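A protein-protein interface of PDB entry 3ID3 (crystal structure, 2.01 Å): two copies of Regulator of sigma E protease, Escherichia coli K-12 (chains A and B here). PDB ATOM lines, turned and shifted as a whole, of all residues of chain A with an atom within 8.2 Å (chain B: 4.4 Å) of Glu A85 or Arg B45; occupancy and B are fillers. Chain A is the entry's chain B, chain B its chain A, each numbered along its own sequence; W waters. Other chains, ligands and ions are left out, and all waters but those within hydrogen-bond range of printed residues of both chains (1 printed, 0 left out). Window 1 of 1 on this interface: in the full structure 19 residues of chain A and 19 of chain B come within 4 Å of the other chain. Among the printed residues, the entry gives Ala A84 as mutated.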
ATOM      1  N   ILE A   2      -6.007  23.174  24.214  1.00  0.00           N
ATOM      2  CA  ILE A   2      -7.353  22.742  24.603  1.00  0.00           C
ATOM      3  C   ILE A   2      -7.667  21.423  23.928  1.00  0.00           C
ATOM      4  O   ILE A   2      -7.565  21.300  22.700  1.00  0.00           O
ATOM      5  CB  ILE A   2      -8.443  23.752  24.192  1.00  0.00           C
ATOM      6  CG1 ILE A   2      -8.260  25.072  24.931  1.00  0.00           C
ATOM      7  CG2 ILE A   2      -9.824  23.186  24.473  1.00  0.00           C
ATOM      8  CD1 ILE A   2      -9.097  26.186  24.359  1.00  0.00           C
ATOM      9  N   GLU A   3      -8.066  20.441  24.730  1.00  0.00           N
ATOM     10  CA  GLU A   3      -8.320  19.094  24.228  1.00  0.00           C
ATOM     11  C   GLU A   3      -9.699  18.997  23.584  1.00  0.00           C
ATOM     12  O   GLU A   3     -10.645  19.628  24.049  1.00  0.00           O
ATOM     13  CB  GLU A   3      -8.203  18.091  25.374  1.00  0.00           C
ATOM     14  CG  GLU A   3      -7.588  16.761  24.984  1.00  0.00           C
ATOM     15  CD  GLU A   3      -7.168  15.955  26.193  1.00  0.00           C
ATOM     16  OE1 GLU A   3      -6.604  14.852  26.016  1.00  0.00           O
ATOM     17  OE2 GLU A   3      -7.406  16.432  27.326  1.00  0.00           O
ATOM     18  N   PRO A   4      -9.817  18.203  22.507  1.00  0.00           N
ATOM     19  CA  PRO A   4     -11.107  18.045  21.825  1.00  0.00           C
ATOM     20  C   PRO A   4     -12.039  17.105  22.607  1.00  0.00           C
ATOM     21  O   PRO A   4     -12.575  16.145  22.044  1.00  0.00           O
ATOM     22  CB  PRO A   4     -10.722  17.414  20.475  1.00  0.00           C
ATOM     23  CG  PRO A   4      -9.225  17.167  20.521  1.00  0.00           C
ATOM     24  CD  PRO A   4      -8.781  17.323  21.940  1.00  0.00           C
ATOM     25  N   VAL A   5     -12.213  17.392  23.894  1.00  0.00           N
ATOM     26  CA  VAL A   5     -13.012  16.581  24.788  1.00  0.00           C
ATOM     27  C   VAL A   5     -14.068  17.485  25.403  1.00  0.00           C
ATOM     28  O   VAL A   5     -13.748  18.535  25.937  1.00  0.00           O
ATOM     29  CB  VAL A   5     -12.150  15.968  25.911  1.00  0.00           C
ATOM     30  CG1 VAL A   5     -12.979  15.049  26.808  1.00  0.00           C
ATOM     31  CG2 VAL A   5     -10.984  15.190  25.316  1.00  0.00           C
ATOM     32  N   LEU A   6     -15.327  17.075  25.317  1.00  0.00           N
ATOM     33  CA  LEU A   6     -16.430  17.904  25.775  1.00  0.00           C
ATOM     34  C   LEU A   6     -16.517  17.922  27.295  1.00  0.00           C
ATOM     35  O   LEU A   6     -16.466  16.879  27.949  1.00  0.00           O
ATOM     36  CB  LEU A   6     -17.750  17.429  25.179  1.00  0.00           C
ATOM     37  CG  LEU A   6     -17.782  17.249  23.659  1.00  0.00           C
ATOM     38  CD1 LEU A   6     -19.212  16.993  23.174  1.00  0.00           C
ATOM     39  CD2 LEU A   6     -17.190  18.473  22.985  1.00  0.00           C
ATOM     40  N   GLU A   7     -16.620  19.128  27.843  1.00  0.00           N
ATOM     41  CA  GLU A   7     -16.882  19.333  29.261  1.00  0.00           C
ATOM     42  C   GLU A   7     -18.387  19.454  29.493  1.00  0.00           C
ATOM     43  O   GLU A   7     -18.907  19.025  30.526  1.00  0.00           O
ATOM     44  CB  GLU A   7     -16.189  20.613  29.742  1.00  0.00           C
ATOM     45  CG  GLU A   7     -16.215  20.797  31.249  1.00  0.00           C
ATOM     46  CD  GLU A   7     -15.306  19.810  31.959  1.00  0.00           C
ATOM     47  OE1 GLU A   7     -14.116  20.125  32.155  1.00  0.00           O
ATOM     48  OE2 GLU A   7     -15.780  18.717  32.319  1.00  0.00           O
ATOM     49  N   ASN A   8     -19.088  20.046  28.530  1.00  0.00           N
ATOM     50  CA  ASN A   8     -20.509  20.313  28.691  1.00  0.00           C
ATOM     51  C   ASN A   8     -21.243  20.361  27.352  1.00  0.00           C
ATOM     52  O   ASN A   8     -20.720  20.888  26.370  1.00  0.00           O
ATOM     53  CB  ASN A   8     -20.725  21.647  29.412  1.00  0.00           C
ATOM     54  CG  ASN A   8     -22.196  21.950  29.643  1.00  0.00           C
ATOM     55  OD1 ASN A   8     -22.839  21.332  30.500  1.00  0.00           O
ATOM     56  ND2 ASN A   8     -22.739  22.905  28.879  1.00  0.00           N
ATOM     57  N   VAL A   9     -22.456  19.823  27.321  1.00  0.00           N
ATOM     58  CA  VAL A   9     -23.295  19.898  26.124  1.00  0.00           C
ATOM     59  C   VAL A   9     -24.554  20.728  26.415  1.00  0.00           C
ATOM     60  O   VAL A   9     -25.286  20.450  27.366  1.00  0.00           O
ATOM     61  CB  VAL A   9     -23.669  18.479  25.596  1.00  0.00           C
ATOM     62  CG1 VAL A   9     -24.616  18.572  24.387  1.00  0.00           C
ATOM     63  CG2 VAL A   9     -22.408  17.693  25.236  1.00  0.00           C
ATOM     64  N   GLN A  10     -24.798  21.744  25.589  1.00  0.00           N
ATOM     65  CA  GLN A  10     -25.958  22.617  25.744  1.00  0.00           C
ATOM     66  C   GLN A  10     -27.224  22.003  25.131  1.00  0.00           C
ATOM     67  O   GLN A  10     -27.156  21.346  24.093  1.00  0.00           O
ATOM     68  CB  GLN A  10     -25.667  23.971  25.092  1.00  0.00           C
ATOM     69  CG  GLN A  10     -24.303  24.549  25.488  1.00  0.00           C
ATOM     70  CD  GLN A  10     -23.837  25.660  24.560  1.00  0.00           C
ATOM     71  OE1 GLN A  10     -24.528  26.022  23.602  1.00  0.00           O
ATOM     72  NE2 GLN A  10     -22.657  26.206  24.839  1.00  0.00           N
ATOM     73  N   PRO A  11     -28.384  22.225  25.773  1.00  0.00           N
ATOM     74  CA  PRO A  11     -29.672  21.704  25.292  1.00  0.00           C
ATOM     75  C   PRO A  11     -30.042  22.314  23.952  1.00  0.00           C
ATOM     76  O   PRO A  11     -29.696  23.469  23.699  1.00  0.00           O
ATOM     77  CB  PRO A  11     -30.671  22.179  26.355  1.00  0.00           C
ATOM     78  CG  PRO A  11     -29.844  22.557  27.540  1.00  0.00           C
ATOM     79  CD  PRO A  11     -28.537  23.032  26.995  1.00  0.00           C
ATOM     80  N   ALA A  15     -24.772  19.826  19.128  1.00  0.00           N
ATOM     81  CA  ALA A  15     -24.135  18.745  19.886  1.00  0.00           C
ATOM     82  C   ALA A  15     -25.132  17.811  20.582  1.00  0.00           C
ATOM     83  O   ALA A  15     -24.967  16.590  20.541  1.00  0.00           O
ATOM     84  CB  ALA A  15     -23.124  19.296  20.872  1.00  0.00           C
ATOM     85  N   GLN A  21     -22.047  13.834  24.300  1.00  0.00           N
ATOM     86  CA  GLN A  21     -22.113  13.917  25.754  1.00  0.00           C
ATOM     87  C   GLN A  21     -20.787  14.380  26.340  1.00  0.00           C
ATOM     88  O   GLN A  21     -19.725  14.184  25.731  1.00  0.00           O
ATOM     89  CB  GLN A  21     -22.459  12.550  26.352  1.00  0.00           C
ATOM     90  CG  GLN A  21     -23.867  12.091  26.088  1.00  0.00           C
ATOM     91  CD  GLN A  21     -24.053  10.619  26.385  1.00  0.00           C
ATOM     92  OE1 GLN A  21     -25.051  10.022  25.985  1.00  0.00           O
ATOM     93  NE2 GLN A  21     -23.085  10.023  27.082  1.00  0.00           N
ATOM     94  N   ALA A  22     -20.862  14.979  27.531  1.00  0.00           N
ATOM     95  CA  ALA A  22     -19.665  15.339  28.287  1.00  0.00           C
ATOM     96  C   ALA A  22     -18.757  14.118  28.388  1.00  0.00           C
ATOM     97  O   ALA A  22     -19.231  13.010  28.656  1.00  0.00           O
ATOM     98  CB  ALA A  22     -20.040  15.854  29.687  1.00  0.00           C
ATOM     99  N   GLY A  23     -17.466  14.310  28.157  1.00  0.00           N
ATOM    100  CA  GLY A  23     -16.523  13.209  28.223  1.00  0.00           C
ATOM    101  C   GLY A  23     -16.202  12.634  26.861  1.00  0.00           C
ATOM    102  O   GLY A  23     -15.211  11.927  26.699  1.00  0.00           O
ATOM    103  N   ASP A  24     -17.046  12.930  25.874  1.00  0.00           N
ATOM    104  CA  ASP A  24     -16.800  12.437  24.525  1.00  0.00           C
ATOM    105  C   ASP A  24     -15.580  13.127  23.922  1.00  0.00           C
ATOM    106  O   ASP A  24     -15.394  14.323  24.089  1.00  0.00           O
ATOM    107  CB  ASP A  24     -18.032  12.658  23.640  1.00  0.00           C
ATOM    108  CG  ASP A  24     -19.165  11.691  23.954  1.00  0.00           C
ATOM    109  OD1 ASP A  24     -18.937  10.690  24.677  1.00  0.00           O
ATOM    110  OD2 ASP A  24     -20.284  11.925  23.457  1.00  0.00           O
ATOM    111  N   TRP A  37      -9.070  21.252  19.825  1.00  0.00           N
ATOM    112  CA  TRP A  37     -10.405  21.831  19.801  1.00  0.00           C
ATOM    113  C   TRP A  37     -10.553  22.869  18.693  1.00  0.00           C
ATOM    114  O   TRP A  37     -11.592  22.944  18.048  1.00  0.00           O
ATOM    115  CB  TRP A  37     -10.688  22.478  21.150  1.00  0.00           C
ATOM    116  CG  TRP A  37     -12.048  23.077  21.319  1.00  0.00           C
ATOM    117  CD1 TRP A  37     -12.340  24.401  21.467  1.00  0.00           C
ATOM    118  CD2 TRP A  37     -13.296  22.384  21.403  1.00  0.00           C
ATOM    119  NE1 TRP A  37     -13.685  24.579  21.632  1.00  0.00           N
ATOM    120  CE2 TRP A  37     -14.305  23.353  21.597  1.00  0.00           C
ATOM    121  CE3 TRP A  37     -13.665  21.040  21.325  1.00  0.00           C
ATOM    122  CZ2 TRP A  37     -15.653  23.027  21.725  1.00  0.00           C
ATOM    123  CZ3 TRP A  37     -15.019  20.713  21.442  1.00  0.00           C
ATOM    124  CH2 TRP A  37     -15.993  21.702  21.640  1.00  0.00           C
ATOM    125  N   LYS A  72     -26.868  30.500  16.392  1.00  0.00           N
ATOM    126  CA  LYS A  72     -27.275  30.736  17.773  1.00  0.00           C
ATOM    127  C   LYS A  72     -28.269  31.892  17.805  1.00  0.00           C
ATOM    128  O   LYS A  72     -28.114  32.853  17.059  1.00  0.00           O
ATOM    129  CB  LYS A  72     -26.057  31.104  18.618  1.00  0.00           C
ATOM    130  CG  LYS A  72     -25.140  29.951  18.934  1.00  0.00           C
ATOM    131  CD  LYS A  72     -25.447  29.396  20.306  1.00  0.00           C
ATOM    132  CE  LYS A  72     -24.414  28.375  20.730  1.00  0.00           C
ATOM    133  NZ  LYS A  72     -24.339  28.290  22.207  1.00  0.00           N
ATOM    134  N   VAL A  82     -21.047  24.774  17.870  1.00  0.00           N
ATOM    135  CA  VAL A  82     -21.056  23.390  18.342  1.00  0.00           C
ATOM    136  C   VAL A  82     -22.221  23.068  19.287  1.00  0.00           C
ATOM    137  O   VAL A  82     -22.868  22.024  19.159  1.00  0.00           O
ATOM    138  CB  VAL A  82     -19.744  23.056  19.092  1.00  0.00           C
ATOM    139  CG1 VAL A  82     -19.769  21.628  19.597  1.00  0.00           C
ATOM    140  CG2 VAL A  82     -18.527  23.303  18.206  1.00  0.00           C
ATOM    141  N   GLY A  83     -22.475  23.965  20.236  1.00  0.00           N
ATOM    142  CA  GLY A  83     -23.411  23.707  21.321  1.00  0.00           C
ATOM    143  C   GLY A  83     -22.764  22.987  22.500  1.00  0.00           C
ATOM    144  O   GLY A  83     -23.443  22.288  23.252  1.00  0.00           O
ATOM    145  N   ALA A  84     -21.451  23.152  22.652  1.00  0.00           N
ATOM    146  CA  ALA A  84     -20.715  22.512  23.745  1.00  0.00           C
ATOM    147  C   ALA A  84     -19.463  23.280  24.145  1.00  0.00           C
ATOM    148  O   ALA A  84     -18.906  24.024  23.336  1.00  0.00           O
ATOM    149  CB  ALA A  84     -20.331  21.111  23.359  1.00  0.00           C
ATOM    150  N   GLU A  85     -19.016  23.063  25.387  1.00  0.00           N
ATOM    151  CA  GLU A  85     -17.757  23.617  25.899  1.00  0.00           C
ATOM    152  C   GLU A  85     -16.699  22.520  26.052  1.00  0.00           C
ATOM    153  O   GLU A  85     -17.036  21.371  26.339  1.00  0.00           O
ATOM    154  CB  GLU A  85     -17.987  24.305  27.243  1.00  0.00           C
ATOM    155  CG  GLU A  85     -18.712  25.651  27.140  1.00  0.00           C
ATOM    156  CD  GLU A  85     -20.226  25.530  27.177  1.00  0.00           C
ATOM    157  OE1 GLU A  85     -20.760  24.407  27.378  1.00  0.00           O
ATOM    158  OE2 GLU A  85     -20.892  26.575  27.015  1.00  0.00           O
ATOM    159  N   PRO A  86     -15.418  22.871  25.874  1.00  0.00           N
ATOM    160  CA  PRO A  86     -14.354  21.867  25.915  1.00  0.00           C
ATOM    161  C   PRO A  86     -13.775  21.742  27.317  1.00  0.00           C
ATOM    162  O   PRO A  86     -13.903  22.664  28.123  1.00  0.00           O
ATOM    163  CB  PRO A  86     -13.269  22.472  25.018  1.00  0.00           C
ATOM    164  CG  PRO A  86     -13.573  23.974  24.951  1.00  0.00           C
ATOM    165  CD  PRO A  86     -14.881  24.228  25.666  1.00  0.00           C
ATOM    166  N   LYS A  87     -13.150  20.609  27.601  1.00  0.00           N
ATOM    167  CA  LYS A  87     -12.356  20.452  28.811  1.00  0.00           C
ATOM    168  C   LYS A  87     -11.040  21.215  28.637  1.00  0.00           C
ATOM    169  O   LYS A  87     -10.517  21.318  27.530  1.00  0.00           O
ATOM    170  CB  LYS A  87     -12.050  18.980  29.077  1.00  0.00           C
ATOM    171  CG  LYS A  87     -13.224  18.135  29.568  1.00  0.00           C
ATOM    172  CD  LYS A  87     -12.696  16.781  30.081  1.00  0.00           C
ATOM    173  CE  LYS A  87     -13.540  16.203  31.217  1.00  0.00           C
ATOM    174  NZ  LYS A  87     -14.853  15.668  30.770  1.00  0.00           N
ATOM    175  N   VAL A  88     -10.508  21.740  29.732  1.00  0.00           N
ATOM    176  CA  VAL A  88      -9.198  22.370  29.711  1.00  0.00           C
ATOM    177  C   VAL A  88      -8.302  21.724  30.772  1.00  0.00           C
ATOM    178  O   VAL A  88      -8.785  21.305  31.825  1.00  0.00           O
ATOM    179  CB  VAL A  88      -9.300  23.892  29.936  1.00  0.00           C
ATOM    180  CG1 VAL A  88      -7.924  24.508  29.883  1.00  0.00           C
ATOM    181  CG2 VAL A  88     -10.214  24.526  28.880  1.00  0.00           C
ATOM    182  N   ILE A  89      -7.006  21.631  30.482  1.00  0.00           N
ATOM    183  CA  ILE A  89      -6.049  20.977  31.378  1.00  0.00           C
ATOM    184  C   ILE A  89      -6.347  21.204  32.863  1.00  0.00           C
ATOM    185  O   ILE A  89      -6.467  22.342  33.329  1.00  0.00           O
ATOM    186  CB  ILE A  89      -4.596  21.410  31.076  1.00  0.00           C
ATOM    187  CG1 ILE A  89      -3.628  20.748  32.062  1.00  0.00           C
ATOM    188  CG2 ILE A  89      -4.459  22.922  31.131  1.00  0.00           C
ATOM    189  CD1 ILE A  89      -3.676  19.231  32.048  1.00  0.00           C
ATOM    190  N   GLN B  10     -23.924  33.977  25.496  1.00  0.00           N
ATOM    191  CA  GLN B  10     -25.161  33.250  25.804  1.00  0.00           C
ATOM    192  C   GLN B  10     -25.997  34.000  26.854  1.00  0.00           C
ATOM    193  O   GLN B  10     -25.440  34.602  27.769  1.00  0.00           O
ATOM    194  CB  GLN B  10     -24.837  31.839  26.308  1.00  0.00           C
ATOM    195  CG  GLN B  10     -23.835  31.085  25.438  1.00  0.00           C
ATOM    196  CD  GLN B  10     -23.194  29.902  26.143  1.00  0.00           C
ATOM    197  OE1 GLN B  10     -23.487  29.624  27.304  1.00  0.00           O
ATOM    198  NE2 GLN B  10     -22.302  29.198  25.434  1.00  0.00           N
ATOM    199  N   VAL B  41     -10.161  30.612  29.898  1.00  0.00           N
ATOM    200  CA  VAL B  41     -11.022  29.484  30.259  1.00  0.00           C
ATOM    201  C   VAL B  41     -10.526  28.741  31.520  1.00  0.00           C
ATOM    202  O   VAL B  41     -11.328  28.376  32.376  1.00  0.00           O
ATOM    203  CB  VAL B  41     -11.233  28.522  29.073  1.00  0.00           C
ATOM    204  CG1 VAL B  41     -12.044  27.305  29.502  1.00  0.00           C
ATOM    205  CG2 VAL B  41     -11.934  29.245  27.922  1.00  0.00           C
ATOM    206  N   MET B  42      -9.219  28.528  31.639  1.00  0.00           N
ATOM    207  CA  MET B  42      -8.666  27.884  32.829  1.00  0.00           C
ATOM    208  C   MET B  42      -9.055  28.667  34.090  1.00  0.00           C
ATOM    209  O   MET B  42      -9.474  28.090  35.083  1.00  0.00           O
ATOM    210  CB  MET B  42      -7.136  27.764  32.735  1.00  0.00           C
ATOM    211  CG  MET B  42      -6.650  26.505  32.031  1.00  0.00           C
ATOM    212  SD  MET B  42      -4.845  26.313  31.976  1.00  0.00           S
ATOM    213  CE  MET B  42      -4.372  27.795  31.082  1.00  0.00           C
ATOM    214  N   LEU B  43      -8.907  29.986  34.036  1.00  0.00           N
ATOM    215  CA  LEU B  43      -9.236  30.842  35.165  1.00  0.00           C
ATOM    216  C   LEU B  43     -10.716  30.729  35.522  1.00  0.00           C
ATOM    217  O   LEU B  43     -11.080  30.620  36.694  1.00  0.00           O
ATOM    218  CB  LEU B  43      -8.846  32.299  34.863  1.00  0.00           C
ATOM    219  CG  LEU B  43      -7.343  32.561  34.739  1.00  0.00           C
ATOM    220  CD1 LEU B  43      -7.062  33.939  34.163  1.00  0.00           C
ATOM    221  CD2 LEU B  43      -6.649  32.388  36.093  1.00  0.00           C
ATOM    222  N   VAL B  44     -11.568  30.748  34.499  1.00  0.00           N
ATOM    223  CA  VAL B  44     -13.011  30.616  34.684  1.00  0.00           C
ATOM    224  C   VAL B  44     -13.380  29.275  35.314  1.00  0.00           C
ATOM    225  O   VAL B  44     -14.150  29.215  36.280  1.00  0.00           O
ATOM    226  CB  VAL B  44     -13.761  30.793  33.339  1.00  0.00           C
ATOM    227  CG1 VAL B  44     -15.204  30.389  33.491  1.00  0.00           C
ATOM    228  CG2 VAL B  44     -13.645  32.242  32.857  1.00  0.00           C
ATOM    229  N   ARG B  45     -12.839  28.197  34.759  1.00  0.00           N
ATOM    230  CA  ARG B  45     -13.019  26.862  35.319  1.00  0.00           C
ATOM    231  C   ARG B  45     -12.621  26.801  36.787  1.00  0.00           C
ATOM    232  O   ARG B  45     -13.305  26.185  37.593  1.00  0.00           O
ATOM    233  CB  ARG B  45     -12.165  25.848  34.545  1.00  0.00           C
ATOM    234  CG  ARG B  45     -12.651  25.597  33.135  1.00  0.00           C
ATOM    235  CD  ARG B  45     -13.850  24.657  33.108  1.00  0.00           C
ATOM    236  NE  ARG B  45     -14.693  24.943  31.957  1.00  0.00           N
ATOM    237  CZ  ARG B  45     -14.375  24.646  30.705  1.00  0.00           C
ATOM    238  NH1 ARG B  45     -15.203  24.963  29.719  1.00  0.00           N
ATOM    239  NH2 ARG B  45     -13.228  24.036  30.440  1.00  0.00           N
ATOM    240  N   ASP B  46     -11.494  27.425  37.124  1.00  0.00           N
ATOM    241  CA  ASP B  46     -10.933  27.292  38.469  1.00  0.00           C
ATOM    242  C   ASP B  46     -11.630  28.181  39.490  1.00  0.00           C
ATOM    243  O   ASP B  46     -11.355  28.080  40.675  1.00  0.00           O
ATOM    244  CB  ASP B  46      -9.437  27.607  38.468  1.00  0.00           C
ATOM    245  CG  ASP B  46      -8.593  26.463  37.917  1.00  0.00           C
ATOM    246  OD1 ASP B  46      -9.143  25.368  37.665  1.00  0.00           O
ATOM    247  OD2 ASP B  46      -7.373  26.662  37.735  1.00  0.00           O
ATOM    248  N   ASN B  47     -12.524  29.050  39.029  1.00  0.00           N
ATOM    249  CA  ASN B  47     -13.060  30.098  39.893  1.00  0.00           C
ATOM    250  C   ASN B  47     -14.578  30.272  39.895  1.00  0.00           C
ATOM    251  O   ASN B  47     -15.068  31.398  39.804  1.00  0.00           O
ATOM    252  CB  ASN B  47     -12.358  31.426  39.590  1.00  0.00           C
ATOM    253  CG  ASN B  47     -10.913  31.427  40.056  1.00  0.00           C
ATOM    254  OD1 ASN B  47     -10.642  31.548  41.252  1.00  0.00           O
ATOM    255  ND2 ASN B  47      -9.977  31.281  39.119  1.00  0.00           N
ATOM    256  N   PRO B  48     -15.322  29.154  40.032  1.00  0.00           N
ATOM    257  CA  PRO B  48     -16.782  29.224  40.166  1.00  0.00           C
ATOM    258  C   PRO B  48     -17.152  30.112  41.356  1.00  0.00           C
ATOM    259  O   PRO B  48     -16.595  29.906  42.438  1.00  0.00           O
ATOM    260  CB  PRO B  48     -17.187  27.767  40.479  1.00  0.00           C
ATOM    261  CG  PRO B  48     -16.009  26.935  40.178  1.00  0.00           C
ATOM    262  CD  PRO B  48     -14.799  27.796  40.265  1.00  0.00           C
ATOM    263  N   LYS B  72     -23.406  25.260  34.979  1.00  0.00           N
ATOM    264  CA  LYS B  72     -24.337  25.116  33.864  1.00  0.00           C
ATOM    265  C   LYS B  72     -25.410  24.104  34.249  1.00  0.00           C
ATOM    266  O   LYS B  72     -25.108  23.102  34.899  1.00  0.00           O
ATOM    267  CB  LYS B  72     -23.597  24.608  32.624  1.00  0.00           C
ATOM    268  CG  LYS B  72     -22.733  25.643  31.932  1.00  0.00           C
ATOM    269  CD  LYS B  72     -23.477  26.277  30.775  1.00  0.00           C
ATOM    270  CE  LYS B  72     -22.569  27.171  29.954  1.00  0.00           C
ATOM    271  NZ  LYS B  72     -23.062  27.296  28.554  1.00  0.00           N
ATOM    272  N   ILE B  79     -16.816  23.248  38.607  1.00  0.00           N
ATOM    273  CA  ILE B  79     -16.076  24.193  37.781  1.00  0.00           C
ATOM    274  C   ILE B  79     -16.963  25.328  37.302  1.00  0.00           C
ATOM    275  O   ILE B  79     -18.192  25.226  37.340  1.00  0.00           O
ATOM    276  CB  ILE B  79     -15.473  23.508  36.542  1.00  0.00           C
ATOM    277  CG1 ILE B  79     -16.566  22.813  35.730  1.00  0.00           C
ATOM    278  CG2 ILE B  79     -14.387  22.515  36.951  1.00  0.00           C
ATOM    279  CD1 ILE B  79     -16.044  22.068  34.519  1.00  0.00           C
ATOM    280  N   GLY B  80     -16.328  26.397  36.828  1.00  0.00           N
ATOM    281  CA  GLY B  80     -17.053  27.541  36.308  1.00  0.00           C
ATOM    282  C   GLY B  80     -17.051  27.567  34.794  1.00  0.00           C
ATOM    283  O   GLY B  80     -16.120  27.046  34.158  1.00  0.00           O
ATOM    284  N   PHE B  81     -18.098  28.166  34.224  1.00  0.00           N
ATOM    285  CA  PHE B  81     -18.220  28.372  32.775  1.00  0.00           C
ATOM    286  C   PHE B  81     -18.366  29.860  32.420  1.00  0.00           C
ATOM    287  O   PHE B  81     -18.899  30.647  33.209  1.00  0.00           O
ATOM    288  CB  PHE B  81     -19.434  27.623  32.230  1.00  0.00           C
ATOM    289  CG  PHE B  81     -19.307  26.122  32.290  1.00  0.00           C
ATOM    290  CD1 PHE B  81     -18.801  25.414  31.212  1.00  0.00           C
ATOM    291  CD2 PHE B  81     -19.696  25.420  33.422  1.00  0.00           C
ATOM    292  CE1 PHE B  81     -18.691  24.022  31.262  1.00  0.00           C
ATOM    293  CE2 PHE B  81     -19.589  24.026  33.477  1.00  0.00           C
ATOM    294  CZ  PHE B  81     -19.089  23.334  32.400  1.00  0.00           C
HETATM  295  O   HOH W   1     -12.285  21.781  31.866  1.00  0.00           O
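NE2 of Gln B10 lies close to NE2 of Gln A10 (3.1 Å).
OE2 of Glu A85 is in hydrogen-bond range of NE2 of Gln B10.
The backbone carbonyl oxygen of Pro A86 lies within hydrogen-bond range of the guanidinium group of Arg B45 (2.8 Å).
NZ of Lys B72 is in salt-bridge range of OE2 of Glu A85, 2.8 Å away.
The backbone NH (N) of Gly B80 lies within hydrogen-bond range of the backbone carbonyl oxygen (O) of Arg B45 (3.1 Å).
O of Leu A6 lies within hydrogen-bond range of NZ of Lys A87 (3.5 Å).
N of Glu A7 is in hydrogen-bond range of O of Glu A85.
The side-chain amide nitrogen (ND2) of Asn A8 lies within hydrogen-bond range of the side-chain carboxylate (OE1) of Glu A85 (2.9 Å).
The backbone NH (N) of Gln A10 sits at hydrogen-bond distance from the backbone carbonyl oxygen (O) of Gly A83 (2.8 Å).
The side-chain amide nitrogen of Gln A10 lies within hydrogen-bond range of the side-chain carboxylate of Glu A85 (2.8 Å).
Among the printed residues, merely in contact across the chains: Val A88 with Met B42 (3.2 Å), Val A88 with Val B41 (3.4 Å), Val A88 with Arg B45 (3.4 Å), Glu A7 with Ile B79 (3.5 Å), Ile A89 with Met B42 (3.5 Å), Asn A8 with Phe B81 (3.6 Å), Glu A85 with Arg B45 (3.8 Å), Gln A10 with Lys B72 (3.9 Å), Lys A72 with Gln B10 (3.9 Å), Asn A8 with Lys B72 (3.9 Å) and Lys A87 with Arg B45 (3.9995 Å).
Of the printed residues of chain A, Arg B45 touches Glu A85, Pro A86, Lys A87 and Val A88.
Of the printed residues of chain B, Lys A72 touches Gln B10 (3.9 Å).
Of the printed residues of chain A, Val B41 touches Val A88.
Of the printed residues of chain A, Lys B72 touches Asn A8 (3.9 Å), Gln A10 (3.9 Å) and Glu A85 (2.8 Å).
Of the printed residues of chain A, Ile B79 touches Glu A7.
Printed residues of chain B within 4 Å of Ile A89: Met B42 (3.5 Å).
Hydrophobic or aromatic side chains of chain A within 4 Å of the printed part of chain B: Val A88 and Ile A89.
Of the 13 printed residues of chain B, 7 touch a printed residue of chain A.
Printed residues of chain B that touch a printed residue of chain A: Gln B10, Val B41, Met B42, Arg B45, Lys B72, Ile B79 and Phe B81.
Hydrophobic or aromatic side chains of chain B that line the printed part of chain A: Val B41, Met B42, Ile B79 and Phe B81.
Among the printed residues, 15 pairs touch across the chains.
Among the printed residues, Asp or Glu carboxylates within 4 Å of a Lys or Arg side-chain nitrogen of the other chain: Glu A85 with Lys B72 (2.8 Å).
Gln B10 touches its own counterpart, Gln A10.
Gln A10 touches Lys B72, and with the chains exchanged Lys A72 touches Gln B10.
Positions printed for both chains: 10 and 72.
Of the 15 pairs that touch across the chains among the printed residues, 3 have their exchanged pair printed and touching as well.
Water W1 lies within hydrogen-bond range of the side-chain carboxylate of Glu A7 (2.5 Å), the backbone NH of Val A88 (2.8 Å) and the guanidinium group of Arg B45 (2.8 Å).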
